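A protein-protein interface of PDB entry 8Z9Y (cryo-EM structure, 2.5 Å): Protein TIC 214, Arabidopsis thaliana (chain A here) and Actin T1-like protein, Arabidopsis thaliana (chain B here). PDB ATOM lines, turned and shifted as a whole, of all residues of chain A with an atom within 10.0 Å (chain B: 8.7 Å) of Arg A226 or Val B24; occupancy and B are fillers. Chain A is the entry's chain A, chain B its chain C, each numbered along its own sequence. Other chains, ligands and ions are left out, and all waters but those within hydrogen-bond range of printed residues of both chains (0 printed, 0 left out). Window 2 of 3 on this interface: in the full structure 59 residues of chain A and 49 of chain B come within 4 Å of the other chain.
Printed residues of chain B within 4 Å of Asn A110: Arg B22 (2.8 Å).
No residue of chain B comes within 4 Å of Ala A225.
Of the printed residues of chain B, Arg A226 touches Asp B21, Val B24 and Asn B25.
Printed residues of chain B within 4 Å of Ile A234: Gly B29.
Of chain A, only Arg A226 (3.7 Å) comes within 4 Å of Val B24.
Of the printed residues of chain A, Ile B26 touches Phe A233 (3.4 Å).
Of the printed residues of chain A, Gly B29 touches Ile A230, Phe A233 and Ile A234.
The nearest residue of chain A that does not touch Val B24 is Ile A230 (5.8 Å).
The nearest printed residue of chain B that does not touch Ile A230 is Val B24 (5.8 Å).
Of the 23 printed residues of chain A, 6 touch a printed residue of chain B.
Along chain B the printed residues that touch a printed residue of chain A span positions 21 to 30.
Among the printed residues, 12 pairs touch across the chains.
Among the printed residues, no Asp or Glu carboxylate lies within 4 Å of a Lys or Arg side-chain nitrogen of the other chain.
OD1 of Asp B19 lies within salt-bridge range of NH1 of Arg B22 (3.0 Å).
The side-chain hydroxyl (OG) of Ser B30 sits at hydrogen-bond distance from the backbone carbonyl oxygen (O) of Ile B26.
The side-chain amide nitrogen (ND2) of Asn B25 lies close to the backbone carbonyl oxygen (O) of Asp B21 (3.2 Å).
Among the printed residues, merely in contact across the chains: Arg A226 with Asp B21, Arg A226 with Val B24, Arg A226 with Asn B25, Ser A229 with Asn B25, Ile A230 with Asn B25, Ile A230 with Ile B28, Ile A230 with Gly B29, Phe A233 with Ile B26, Phe A233 with Gly B29, Phe A233 with Ser B30 and Ile A234 with Gly B29.
The side-chain amide oxygen (OD1) of Asn A110 lies within hydrogen-bond range of the guanidinium group (NH1) of Arg B22.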
ATOM      1  N   LEU A  46      19.710  20.260  19.171  1.00  0.00           N
ATOM      2  CA  LEU A  46      21.060  20.756  18.912  1.00  0.00           C
ATOM      3  C   LEU A  46      21.031  22.205  18.425  1.00  0.00           C
ATOM      4  O   LEU A  46      21.955  22.983  18.700  1.00  0.00           O
ATOM      5  CB  LEU A  46      21.763  19.844  17.903  1.00  0.00           C
ATOM      6  CG  LEU A  46      23.034  20.315  17.193  1.00  0.00           C
ATOM      7  CD1 LEU A  46      23.980  19.144  16.996  1.00  0.00           C
ATOM      8  CD2 LEU A  46      22.708  20.946  15.851  1.00  0.00           C
ATOM      9  N   ARG A  47      19.987  22.576  17.681  1.00  0.00           N
ATOM     10  CA  ARG A  47      19.831  23.970  17.277  1.00  0.00           C
ATOM     11  C   ARG A  47      19.566  24.867  18.481  1.00  0.00           C
ATOM     12  O   ARG A  47      19.817  26.077  18.431  1.00  0.00           O
ATOM     13  CB  ARG A  47      18.707  24.103  16.246  1.00  0.00           C
ATOM     14  CG  ARG A  47      18.471  25.531  15.771  1.00  0.00           C
ATOM     15  CD  ARG A  47      18.145  25.592  14.291  1.00  0.00           C
ATOM     16  NE  ARG A  47      17.735  26.927  13.871  1.00  0.00           N
ATOM     17  CZ  ARG A  47      18.557  27.962  13.752  1.00  0.00           C
ATOM     18  NH1 ARG A  47      19.851  27.851  14.001  1.00  0.00           N
ATOM     19  NH2 ARG A  47      18.067  29.138  13.369  1.00  0.00           N
ATOM     20  N   VAL A  50      23.190  25.577  19.399  1.00  0.00           N
ATOM     21  CA  VAL A  50      24.072  26.268  18.457  1.00  0.00           C
ATOM     22  C   VAL A  50      24.089  27.765  18.747  1.00  0.00           C
ATOM     23  O   VAL A  50      25.129  28.421  18.605  1.00  0.00           O
ATOM     24  CB  VAL A  50      23.686  25.993  16.988  1.00  0.00           C
ATOM     25  CG1 VAL A  50      22.252  26.339  16.725  1.00  0.00           C
ATOM     26  CG2 VAL A  50      24.577  26.778  16.051  1.00  0.00           C
ATOM     27  N   MET A  51      22.957  28.327  19.172  1.00  0.00           N
ATOM     28  CA  MET A  51      22.840  29.750  19.463  1.00  0.00           C
ATOM     29  C   MET A  51      22.654  29.997  20.961  1.00  0.00           C
ATOM     30  O   MET A  51      21.949  30.923  21.369  1.00  0.00           O
ATOM     31  CB  MET A  51      21.692  30.355  18.649  1.00  0.00           C
ATOM     32  CG  MET A  51      21.584  31.894  18.611  1.00  0.00           C
ATOM     33  SD  MET A  51      23.103  32.883  18.596  1.00  0.00           S
ATOM     34  CE  MET A  51      24.085  32.096  17.318  1.00  0.00           C
ATOM     35  N   PHE A 106      14.792  23.902   6.317  1.00  0.00           N
ATOM     36  CA  PHE A 106      16.188  24.060   5.919  1.00  0.00           C
ATOM     37  C   PHE A 106      16.412  25.388   5.199  1.00  0.00           C
ATOM     38  O   PHE A 106      17.166  26.258   5.670  1.00  0.00           O
ATOM     39  CB  PHE A 106      16.594  22.881   5.030  1.00  0.00           C
ATOM     40  CG  PHE A 106      17.978  22.991   4.457  1.00  0.00           C
ATOM     41  CD1 PHE A 106      19.092  22.939   5.276  1.00  0.00           C
ATOM     42  CD2 PHE A 106      18.163  23.124   3.091  1.00  0.00           C
ATOM     43  CE1 PHE A 106      20.365  23.032   4.744  1.00  0.00           C
ATOM     44  CE2 PHE A 106      19.431  23.217   2.554  1.00  0.00           C
ATOM     45  CZ  PHE A 106      20.533  23.170   3.381  1.00  0.00           C
ATOM     46  N   ASN A 110      18.290  28.807   6.914  1.00  0.00           N
ATOM     47  CA  ASN A 110      19.388  29.575   6.340  1.00  0.00           C
ATOM     48  C   ASN A 110      19.103  31.071   6.419  1.00  0.00           C
ATOM     49  O   ASN A 110      19.960  31.856   6.839  1.00  0.00           O
ATOM     50  CB  ASN A 110      19.632  29.157   4.894  1.00  0.00           C
ATOM     51  CG  ASN A 110      20.909  29.738   4.345  1.00  0.00           C
ATOM     52  OD1 ASN A 110      20.880  30.640   3.510  1.00  0.00           O
ATOM     53  ND2 ASN A 110      22.042  29.240   4.829  1.00  0.00           N
ATOM     54  N   SER A 218      36.935  26.137  20.426  1.00  0.00           N
ATOM     55  CA  SER A 218      36.200  27.127  19.643  1.00  0.00           C
ATOM     56  C   SER A 218      36.026  26.672  18.201  1.00  0.00           C
ATOM     57  O   SER A 218      35.000  26.971  17.571  1.00  0.00           O
ATOM     58  CB  SER A 218      36.916  28.475  19.695  1.00  0.00           C
ATOM     59  OG  SER A 218      38.307  28.322  19.469  1.00  0.00           O
ATOM     60  N   GLU A 219      37.011  25.947  17.666  1.00  0.00           N
ATOM     61  CA  GLU A 219      36.862  25.374  16.335  1.00  0.00           C
ATOM     62  C   GLU A 219      35.682  24.414  16.291  1.00  0.00           C
ATOM     63  O   GLU A 219      34.888  24.443  15.348  1.00  0.00           O
ATOM     64  CB  GLU A 219      38.151  24.665  15.917  1.00  0.00           C
ATOM     65  CG  GLU A 219      38.238  24.370  14.427  1.00  0.00           C
ATOM     66  CD  GLU A 219      37.773  22.970  14.080  1.00  0.00           C
ATOM     67  OE1 GLU A 219      37.451  22.200  15.009  1.00  0.00           O
ATOM     68  OE2 GLU A 219      37.729  22.639  12.876  1.00  0.00           O
ATOM     69  N   LEU A 220      35.534  23.574  17.320  1.00  0.00           N
ATOM     70  CA  LEU A 220      34.376  22.687  17.385  1.00  0.00           C
ATOM     71  C   LEU A 220      33.086  23.457  17.639  1.00  0.00           C
ATOM     72  O   LEU A 220      32.019  23.046  17.169  1.00  0.00           O
ATOM     73  CB  LEU A 220      34.582  21.627  18.466  1.00  0.00           C
ATOM     74  CG  LEU A 220      33.853  20.301  18.237  1.00  0.00           C
ATOM     75  CD1 LEU A 220      34.345  19.630  16.962  1.00  0.00           C
ATOM     76  CD2 LEU A 220      34.023  19.379  19.434  1.00  0.00           C
ATOM     77  N   ARG A 221      33.158  24.566  18.379  1.00  0.00           N
ATOM     78  CA  ARG A 221      31.964  25.371  18.618  1.00  0.00           C
ATOM     79  C   ARG A 221      31.434  25.967  17.321  1.00  0.00           C
ATOM     80  O   ARG A 221      30.218  26.039  17.112  1.00  0.00           O
ATOM     81  CB  ARG A 221      32.267  26.471  19.636  1.00  0.00           C
ATOM     82  CG  ARG A 221      32.292  25.998  21.084  1.00  0.00           C
ATOM     83  CD  ARG A 221      30.927  25.504  21.548  1.00  0.00           C
ATOM     84  NE  ARG A 221      30.739  24.078  21.304  1.00  0.00           N
ATOM     85  CZ  ARG A 221      31.267  23.112  22.043  1.00  0.00           C
ATOM     86  NH1 ARG A 221      32.023  23.381  23.095  1.00  0.00           N
ATOM     87  NH2 ARG A 221      31.030  21.844  21.719  1.00  0.00           N
ATOM     88  N   ASN A 222      32.332  26.414  16.443  1.00  0.00           N
ATOM     89  CA  ASN A 222      31.906  26.852  15.117  1.00  0.00           C
ATOM     90  C   ASN A 222      31.532  25.672  14.224  1.00  0.00           C
ATOM     91  O   ASN A 222      30.618  25.781  13.393  1.00  0.00           O
ATOM     92  CB  ASN A 222      33.007  27.688  14.462  1.00  0.00           C
ATOM     93  CG  ASN A 222      32.610  28.209  13.093  1.00  0.00           C
ATOM     94  OD1 ASN A 222      32.665  27.485  12.099  1.00  0.00           O
ATOM     95  ND2 ASN A 222      32.207  29.472  13.037  1.00  0.00           N
ATOM     96  N   SER A 223      32.216  24.539  14.389  1.00  0.00           N
ATOM     97  CA  SER A 223      31.966  23.380  13.546  1.00  0.00           C
ATOM     98  C   SER A 223      30.592  22.781  13.798  1.00  0.00           C
ATOM     99  O   SER A 223      29.993  22.226  12.878  1.00  0.00           O
ATOM    100  CB  SER A 223      33.052  22.327  13.766  1.00  0.00           C
ATOM    101  OG  SER A 223      32.739  21.125  13.085  1.00  0.00           O
ATOM    102  N   MET A 224      30.083  22.860  15.029  1.00  0.00           N
ATOM    103  CA  MET A 224      28.738  22.351  15.285  1.00  0.00           C
ATOM    104  C   MET A 224      27.687  23.202  14.578  1.00  0.00           C
ATOM    105  O   MET A 224      26.716  22.670  14.019  1.00  0.00           O
ATOM    106  CB  MET A 224      28.481  22.264  16.793  1.00  0.00           C
ATOM    107  CG  MET A 224      28.295  23.588  17.508  1.00  0.00           C
ATOM    108  SD  MET A 224      26.585  23.868  17.993  1.00  0.00           S
ATOM    109  CE  MET A 224      26.492  22.893  19.492  1.00  0.00           C
ATOM    110  N   ALA A 225      27.885  24.523  14.563  1.00  0.00           N
ATOM    111  CA  ALA A 225      27.028  25.394  13.768  1.00  0.00           C
ATOM    112  C   ALA A 225      27.119  25.040  12.293  1.00  0.00           C
ATOM    113  O   ALA A 225      26.112  25.050  11.577  1.00  0.00           O
ATOM    114  CB  ALA A 225      27.417  26.855  13.990  1.00  0.00           C
ATOM    115  N   ARG A 226      28.329  24.736  11.820  1.00  0.00           N
ATOM    116  CA  ARG A 226      28.493  24.342  10.425  1.00  0.00           C
ATOM    117  C   ARG A 226      27.778  23.028  10.121  1.00  0.00           C
ATOM    118  O   ARG A 226      27.135  22.891   9.074  1.00  0.00           O
ATOM    119  CB  ARG A 226      29.977  24.232  10.082  1.00  0.00           C
ATOM    120  CG  ARG A 226      30.504  25.392   9.259  1.00  0.00           C
ATOM    121  CD  ARG A 226      29.944  25.350   7.850  1.00  0.00           C
ATOM    122  NE  ARG A 226      30.668  26.234   6.944  1.00  0.00           N
ATOM    123  CZ  ARG A 226      31.637  25.838   6.132  1.00  0.00           C
ATOM    124  NH1 ARG A 226      32.028  24.574   6.087  1.00  0.00           N
ATOM    125  NH2 ARG A 226      32.231  26.731   5.346  1.00  0.00           N
ATOM    126  N   ILE A 227      27.872  22.049  11.028  1.00  0.00           N
ATOM    127  CA  ILE A 227      27.387  20.702  10.735  1.00  0.00           C
ATOM    128  C   ILE A 227      25.906  20.521  11.027  1.00  0.00           C
ATOM    129  O   ILE A 227      25.337  19.491  10.636  1.00  0.00           O
ATOM    130  CB  ILE A 227      28.238  19.627  11.458  1.00  0.00           C
ATOM    131  CG1 ILE A 227      28.226  19.719  12.999  1.00  0.00           C
ATOM    132  CG2 ILE A 227      29.674  19.652  10.943  1.00  0.00           C
ATOM    133  CD1 ILE A 227      26.913  19.462  13.734  1.00  0.00           C
ATOM    134  N   PHE A 228      25.264  21.470  11.711  1.00  0.00           N
ATOM    135  CA  PHE A 228      23.808  21.397  11.804  1.00  0.00           C
ATOM    136  C   PHE A 228      23.182  21.399  10.416  1.00  0.00           C
ATOM    137  O   PHE A 228      22.270  20.610  10.135  1.00  0.00           O
ATOM    138  CB  PHE A 228      23.252  22.555  12.627  1.00  0.00           C
ATOM    139  CG  PHE A 228      21.775  22.759  12.441  1.00  0.00           C
ATOM    140  CD1 PHE A 228      20.871  21.822  12.909  1.00  0.00           C
ATOM    141  CD2 PHE A 228      21.293  23.873  11.778  1.00  0.00           C
ATOM    142  CE1 PHE A 228      19.513  21.998  12.731  1.00  0.00           C
ATOM    143  CE2 PHE A 228      19.935  24.054  11.597  1.00  0.00           C
ATOM    144  CZ  PHE A 228      19.045  23.114  12.074  1.00  0.00           C
ATOM    145  N   SER A 229      23.672  22.270   9.530  1.00  0.00           N
ATOM    146  CA  SER A 229      23.167  22.307   8.162  1.00  0.00           C
ATOM    147  C   SER A 229      23.456  21.004   7.429  1.00  0.00           C
ATOM    148  O   SER A 229      22.619  20.520   6.659  1.00  0.00           O
ATOM    149  CB  SER A 229      23.778  23.490   7.412  1.00  0.00           C
ATOM    150  OG  SER A 229      23.485  24.713   8.066  1.00  0.00           O
ATOM    151  N   ILE A 230      24.640  20.427   7.645  1.00  0.00           N
ATOM    152  CA  ILE A 230      24.994  19.176   6.977  1.00  0.00           C
ATOM    153  C   ILE A 230      24.059  18.055   7.416  1.00  0.00           C
ATOM    154  O   ILE A 230      23.562  17.276   6.594  1.00  0.00           O
ATOM    155  CB  ILE A 230      26.466  18.822   7.249  1.00  0.00           C
ATOM    156  CG1 ILE A 230      27.386  19.883   6.642  1.00  0.00           C
ATOM    157  CG2 ILE A 230      26.797  17.446   6.696  1.00  0.00           C
ATOM    158  CD1 ILE A 230      28.718  20.010   7.344  1.00  0.00           C
ATOM    159  N   LEU A 231      23.807  17.957   8.723  1.00  0.00           N
ATOM    160  CA  LEU A 231      22.902  16.929   9.227  1.00  0.00           C
ATOM    161  C   LEU A 231      21.483  17.150   8.721  1.00  0.00           C
ATOM    162  O   LEU A 231      20.779  16.190   8.385  1.00  0.00           O
ATOM    163  CB  LEU A 231      22.930  16.906  10.755  1.00  0.00           C
ATOM    164  CG  LEU A 231      24.231  16.423  11.395  1.00  0.00           C
ATOM    165  CD1 LEU A 231      24.178  16.585  12.904  1.00  0.00           C
ATOM    166  CD2 LEU A 231      24.508  14.977  11.018  1.00  0.00           C
ATOM    167  N   LEU A 232      21.044  18.410   8.660  1.00  0.00           N
ATOM    168  CA  LEU A 232      19.715  18.701   8.136  1.00  0.00           C
ATOM    169  C   LEU A 232      19.603  18.299   6.671  1.00  0.00           C
ATOM    170  O   LEU A 232      18.588  17.734   6.250  1.00  0.00           O
ATOM    171  CB  LEU A 232      19.402  20.186   8.317  1.00  0.00           C
ATOM    172  CG  LEU A 232      17.988  20.652   7.981  1.00  0.00           C
ATOM    173  CD1 LEU A 232      16.968  19.699   8.568  1.00  0.00           C
ATOM    174  CD2 LEU A 232      17.767  22.057   8.512  1.00  0.00           C
ATOM    175  N   PHE A 233      20.641  18.576   5.881  1.00  0.00           N
ATOM    176  CA  PHE A 233      20.639  18.187   4.474  1.00  0.00           C
ATOM    177  C   PHE A 233      20.625  16.670   4.320  1.00  0.00           C
ATOM    178  O   PHE A 233      19.927  16.131   3.452  1.00  0.00           O
ATOM    179  CB  PHE A 233      21.853  18.792   3.771  1.00  0.00           C
ATOM    180  CG  PHE A 233      22.068  18.276   2.379  1.00  0.00           C
ATOM    181  CD1 PHE A 233      21.153  18.546   1.377  1.00  0.00           C
ATOM    182  CD2 PHE A 233      23.187  17.524   2.072  1.00  0.00           C
ATOM    183  CE1 PHE A 233      21.351  18.074   0.097  1.00  0.00           C
ATOM    184  CE2 PHE A 233      23.389  17.047   0.793  1.00  0.00           C
ATOM    185  CZ  PHE A 233      22.469  17.323  -0.196  1.00  0.00           C
ATOM    186  N   ILE A 234      21.398  15.966   5.150  1.00  0.00           N
ATOM    187  CA  ILE A 234      21.414  14.507   5.093  1.00  0.00           C
ATOM    188  C   ILE A 234      20.039  13.945   5.434  1.00  0.00           C
ATOM    189  O   ILE A 234      19.549  13.019   4.776  1.00  0.00           O
ATOM    190  CB  ILE A 234      22.505  13.947   6.024  1.00  0.00           C
ATOM    191  CG1 ILE A 234      23.891  14.230   5.448  1.00  0.00           C
ATOM    192  CG2 ILE A 234      22.315  12.454   6.239  1.00  0.00           C
ATOM    193  CD1 ILE A 234      24.998  14.176   6.474  1.00  0.00           C
ATOM    194  N   ASP B  19      26.476  33.858   0.971  1.00  0.00           N
ATOM    195  CA  ASP B  19      27.477  33.239   1.829  1.00  0.00           C
ATOM    196  C   ASP B  19      27.932  31.918   1.220  1.00  0.00           C
ATOM    197  O   ASP B  19      27.110  31.083   0.831  1.00  0.00           O
ATOM    198  CB  ASP B  19      26.912  33.025   3.231  1.00  0.00           C
ATOM    199  CG  ASP B  19      25.472  32.555   3.215  1.00  0.00           C
ATOM    200  OD1 ASP B  19      24.813  32.704   2.165  1.00  0.00           O
ATOM    201  OD2 ASP B  19      25.000  32.038   4.248  1.00  0.00           O
ATOM    202  N   ALA B  20      29.251  31.731   1.140  1.00  0.00           N
ATOM    203  CA  ALA B  20      29.808  30.592   0.420  1.00  0.00           C
ATOM    204  C   ALA B  20      29.658  29.277   1.174  1.00  0.00           C
ATOM    205  O   ALA B  20      29.752  28.213   0.556  1.00  0.00           O
ATOM    206  CB  ALA B  20      31.285  30.840   0.109  1.00  0.00           C
ATOM    207  N   ASP B  21      29.429  29.321   2.489  1.00  0.00           N
ATOM    208  CA  ASP B  21      29.380  28.088   3.266  1.00  0.00           C
ATOM    209  C   ASP B  21      28.181  27.219   2.914  1.00  0.00           C
ATOM    210  O   ASP B  21      28.169  26.036   3.265  1.00  0.00           O
ATOM    211  CB  ASP B  21      29.362  28.404   4.763  1.00  0.00           C
ATOM    212  CG  ASP B  21      28.534  29.626   5.089  1.00  0.00           C
ATOM    213  OD1 ASP B  21      28.097  30.310   4.143  1.00  0.00           O
ATOM    214  OD2 ASP B  21      28.319  29.902   6.288  1.00  0.00           O
ATOM    215  N   ARG B  22      27.178  27.769   2.227  1.00  0.00           N
ATOM    216  CA  ARG B  22      26.001  26.984   1.873  1.00  0.00           C
ATOM    217  C   ARG B  22      26.343  25.889   0.871  1.00  0.00           C
ATOM    218  O   ARG B  22      25.977  24.722   1.056  1.00  0.00           O
ATOM    219  CB  ARG B  22      24.919  27.904   1.315  1.00  0.00           C
ATOM    220  CG  ARG B  22      24.562  29.029   2.250  1.00  0.00           C
ATOM    221  CD  ARG B  22      23.230  29.635   1.889  1.00  0.00           C
ATOM    222  NE  ARG B  22      23.264  30.388   0.644  1.00  0.00           N
ATOM    223  CZ  ARG B  22      22.640  31.544   0.461  1.00  0.00           C
ATOM    224  NH1 ARG B  22      21.930  32.106   1.425  1.00  0.00           N
ATOM    225  NH2 ARG B  22      22.728  32.148  -0.719  1.00  0.00           N
ATOM    226  N   PHE B  23      27.043  26.251  -0.205  1.00  0.00           N
ATOM    227  CA  PHE B  23      27.408  25.263  -1.213  1.00  0.00           C
ATOM    228  C   PHE B  23      28.422  24.271  -0.661  1.00  0.00           C
ATOM    229  O   PHE B  23      28.387  23.081  -1.004  1.00  0.00           O
ATOM    230  CB  PHE B  23      27.946  25.972  -2.453  1.00  0.00           C
ATOM    231  CG  PHE B  23      27.027  27.038  -2.978  1.00  0.00           C
ATOM    232  CD1 PHE B  23      25.988  26.716  -3.833  1.00  0.00           C
ATOM    233  CD2 PHE B  23      27.199  28.361  -2.609  1.00  0.00           C
ATOM    234  CE1 PHE B  23      25.142  27.695  -4.314  1.00  0.00           C
ATOM    235  CE2 PHE B  23      26.356  29.344  -3.086  1.00  0.00           C
ATOM    236  CZ  PHE B  23      25.325  29.011  -3.940  1.00  0.00           C
ATOM    237  N   VAL B  24      29.328  24.740   0.199  1.00  0.00           N
ATOM    238  CA  VAL B  24      30.257  23.837   0.871  1.00  0.00           C
ATOM    239  C   VAL B  24      29.492  22.827   1.715  1.00  0.00           C
ATOM    240  O   VAL B  24      29.797  21.629   1.704  1.00  0.00           O
ATOM    241  CB  VAL B  24      31.258  24.639   1.723  1.00  0.00           C
ATOM    242  CG1 VAL B  24      32.189  23.701   2.474  1.00  0.00           C
ATOM    243  CG2 VAL B  24      32.050  25.594   0.852  1.00  0.00           C
ATOM    244  N   ASN B  25      28.487  23.295   2.458  1.00  0.00           N
ATOM    245  CA  ASN B  25      27.672  22.392   3.261  1.00  0.00           C
ATOM    246  C   ASN B  25      26.938  21.389   2.386  1.00  0.00           C
ATOM    247  O   ASN B  25      26.850  20.207   2.726  1.00  0.00           O
ATOM    248  CB  ASN B  25      26.679  23.189   4.106  1.00  0.00           C
ATOM    249  CG  ASN B  25      27.338  23.887   5.275  1.00  0.00           C
ATOM    250  OD1 ASN B  25      28.428  23.510   5.702  1.00  0.00           O
ATOM    251  ND2 ASN B  25      26.677  24.910   5.802  1.00  0.00           N
ATOM    252  N   ILE B  26      26.405  21.845   1.251  1.00  0.00           N
ATOM    253  CA  ILE B  26      25.687  20.946   0.349  1.00  0.00           C
ATOM    254  C   ILE B  26      26.615  19.851  -0.165  1.00  0.00           C
ATOM    255  O   ILE B  26      26.273  18.662  -0.152  1.00  0.00           O
ATOM    256  CB  ILE B  26      25.057  21.742  -0.808  1.00  0.00           C
ATOM    257  CG1 ILE B  26      23.823  22.503  -0.323  1.00  0.00           C
ATOM    258  CG2 ILE B  26      24.703  20.820  -1.961  1.00  0.00           C
ATOM    259  CD1 ILE B  26      23.347  23.567  -1.284  1.00  0.00           C
ATOM    260  N   TRP B  27      27.809  20.238  -0.618  1.00  0.00           N
ATOM    261  CA  TRP B  27      28.751  19.259  -1.153  1.00  0.00           C
ATOM    262  C   TRP B  27      29.218  18.285  -0.076  1.00  0.00           C
ATOM    263  O   TRP B  27      29.299  17.071  -0.316  1.00  0.00           O
ATOM    264  CB  TRP B  27      29.940  19.977  -1.789  1.00  0.00           C
ATOM    265  CG  TRP B  27      29.546  20.928  -2.880  1.00  0.00           C
ATOM    266  CD1 TRP B  27      28.382  20.920  -3.593  1.00  0.00           C
ATOM    267  CD2 TRP B  27      30.312  22.032  -3.377  1.00  0.00           C
ATOM    268  NE1 TRP B  27      28.378  21.947  -4.505  1.00  0.00           N
ATOM    269  CE2 TRP B  27      29.551  22.644  -4.392  1.00  0.00           C
ATOM    270  CE3 TRP B  27      31.567  22.560  -3.065  1.00  0.00           C
ATOM    271  CZ2 TRP B  27      30.004  23.757  -5.096  1.00  0.00           C
ATOM    272  CZ3 TRP B  27      32.015  23.666  -3.764  1.00  0.00           C
ATOM    273  CH2 TRP B  27      31.236  24.251  -4.767  1.00  0.00           C
ATOM    274  N   ILE B  28      29.526  18.798   1.118  1.00  0.00           N
ATOM    275  CA  ILE B  28      29.969  17.936   2.209  1.00  0.00           C
ATOM    276  C   ILE B  28      28.864  16.967   2.603  1.00  0.00           C
ATOM    277  O   ILE B  28      29.117  15.785   2.860  1.00  0.00           O
ATOM    278  CB  ILE B  28      30.435  18.787   3.405  1.00  0.00           C
ATOM    279  CG1 ILE B  28      31.752  19.491   3.076  1.00  0.00           C
ATOM    280  CG2 ILE B  28      30.595  17.928   4.649  1.00  0.00           C
ATOM    281  CD1 ILE B  28      32.250  20.394   4.179  1.00  0.00           C
ATOM    282  N   GLY B  29      27.621  17.449   2.654  1.00  0.00           N
ATOM    283  CA  GLY B  29      26.511  16.572   2.978  1.00  0.00           C
ATOM    284  C   GLY B  29      26.296  15.497   1.934  1.00  0.00           C
ATOM    285  O   GLY B  29      25.991  14.352   2.267  1.00  0.00           O
ATOM    286  N   SER B  30      26.450  15.849   0.655  1.00  0.00           N
ATOM    287  CA  SER B  30      26.323  14.844  -0.397  1.00  0.00           C
ATOM    288  C   SER B  30      27.398  13.772  -0.270  1.00  0.00           C
ATOM    289  O   SER B  30      27.109  12.571  -0.372  1.00  0.00           O
ATOM    290  CB  SER B  30      26.387  15.512  -1.770  1.00  0.00           C
ATOM    291  OG  SER B  30      25.163  16.157  -2.077  1.00  0.00           O
ATOM    292  N   ALA B  31      28.647  14.186  -0.035  1.00  0.00           N
ATOM    293  CA  ALA B  31      29.722  13.211   0.130  1.00  0.00           C
ATOM    294  C   ALA B  31      29.487  12.325   1.349  1.00  0.00           C
ATOM    295  O   ALA B  31      29.682  11.103   1.291  1.00  0.00           O
ATOM    296  CB  ALA B  31      31.069  13.926   0.236  1.00  0.00           C
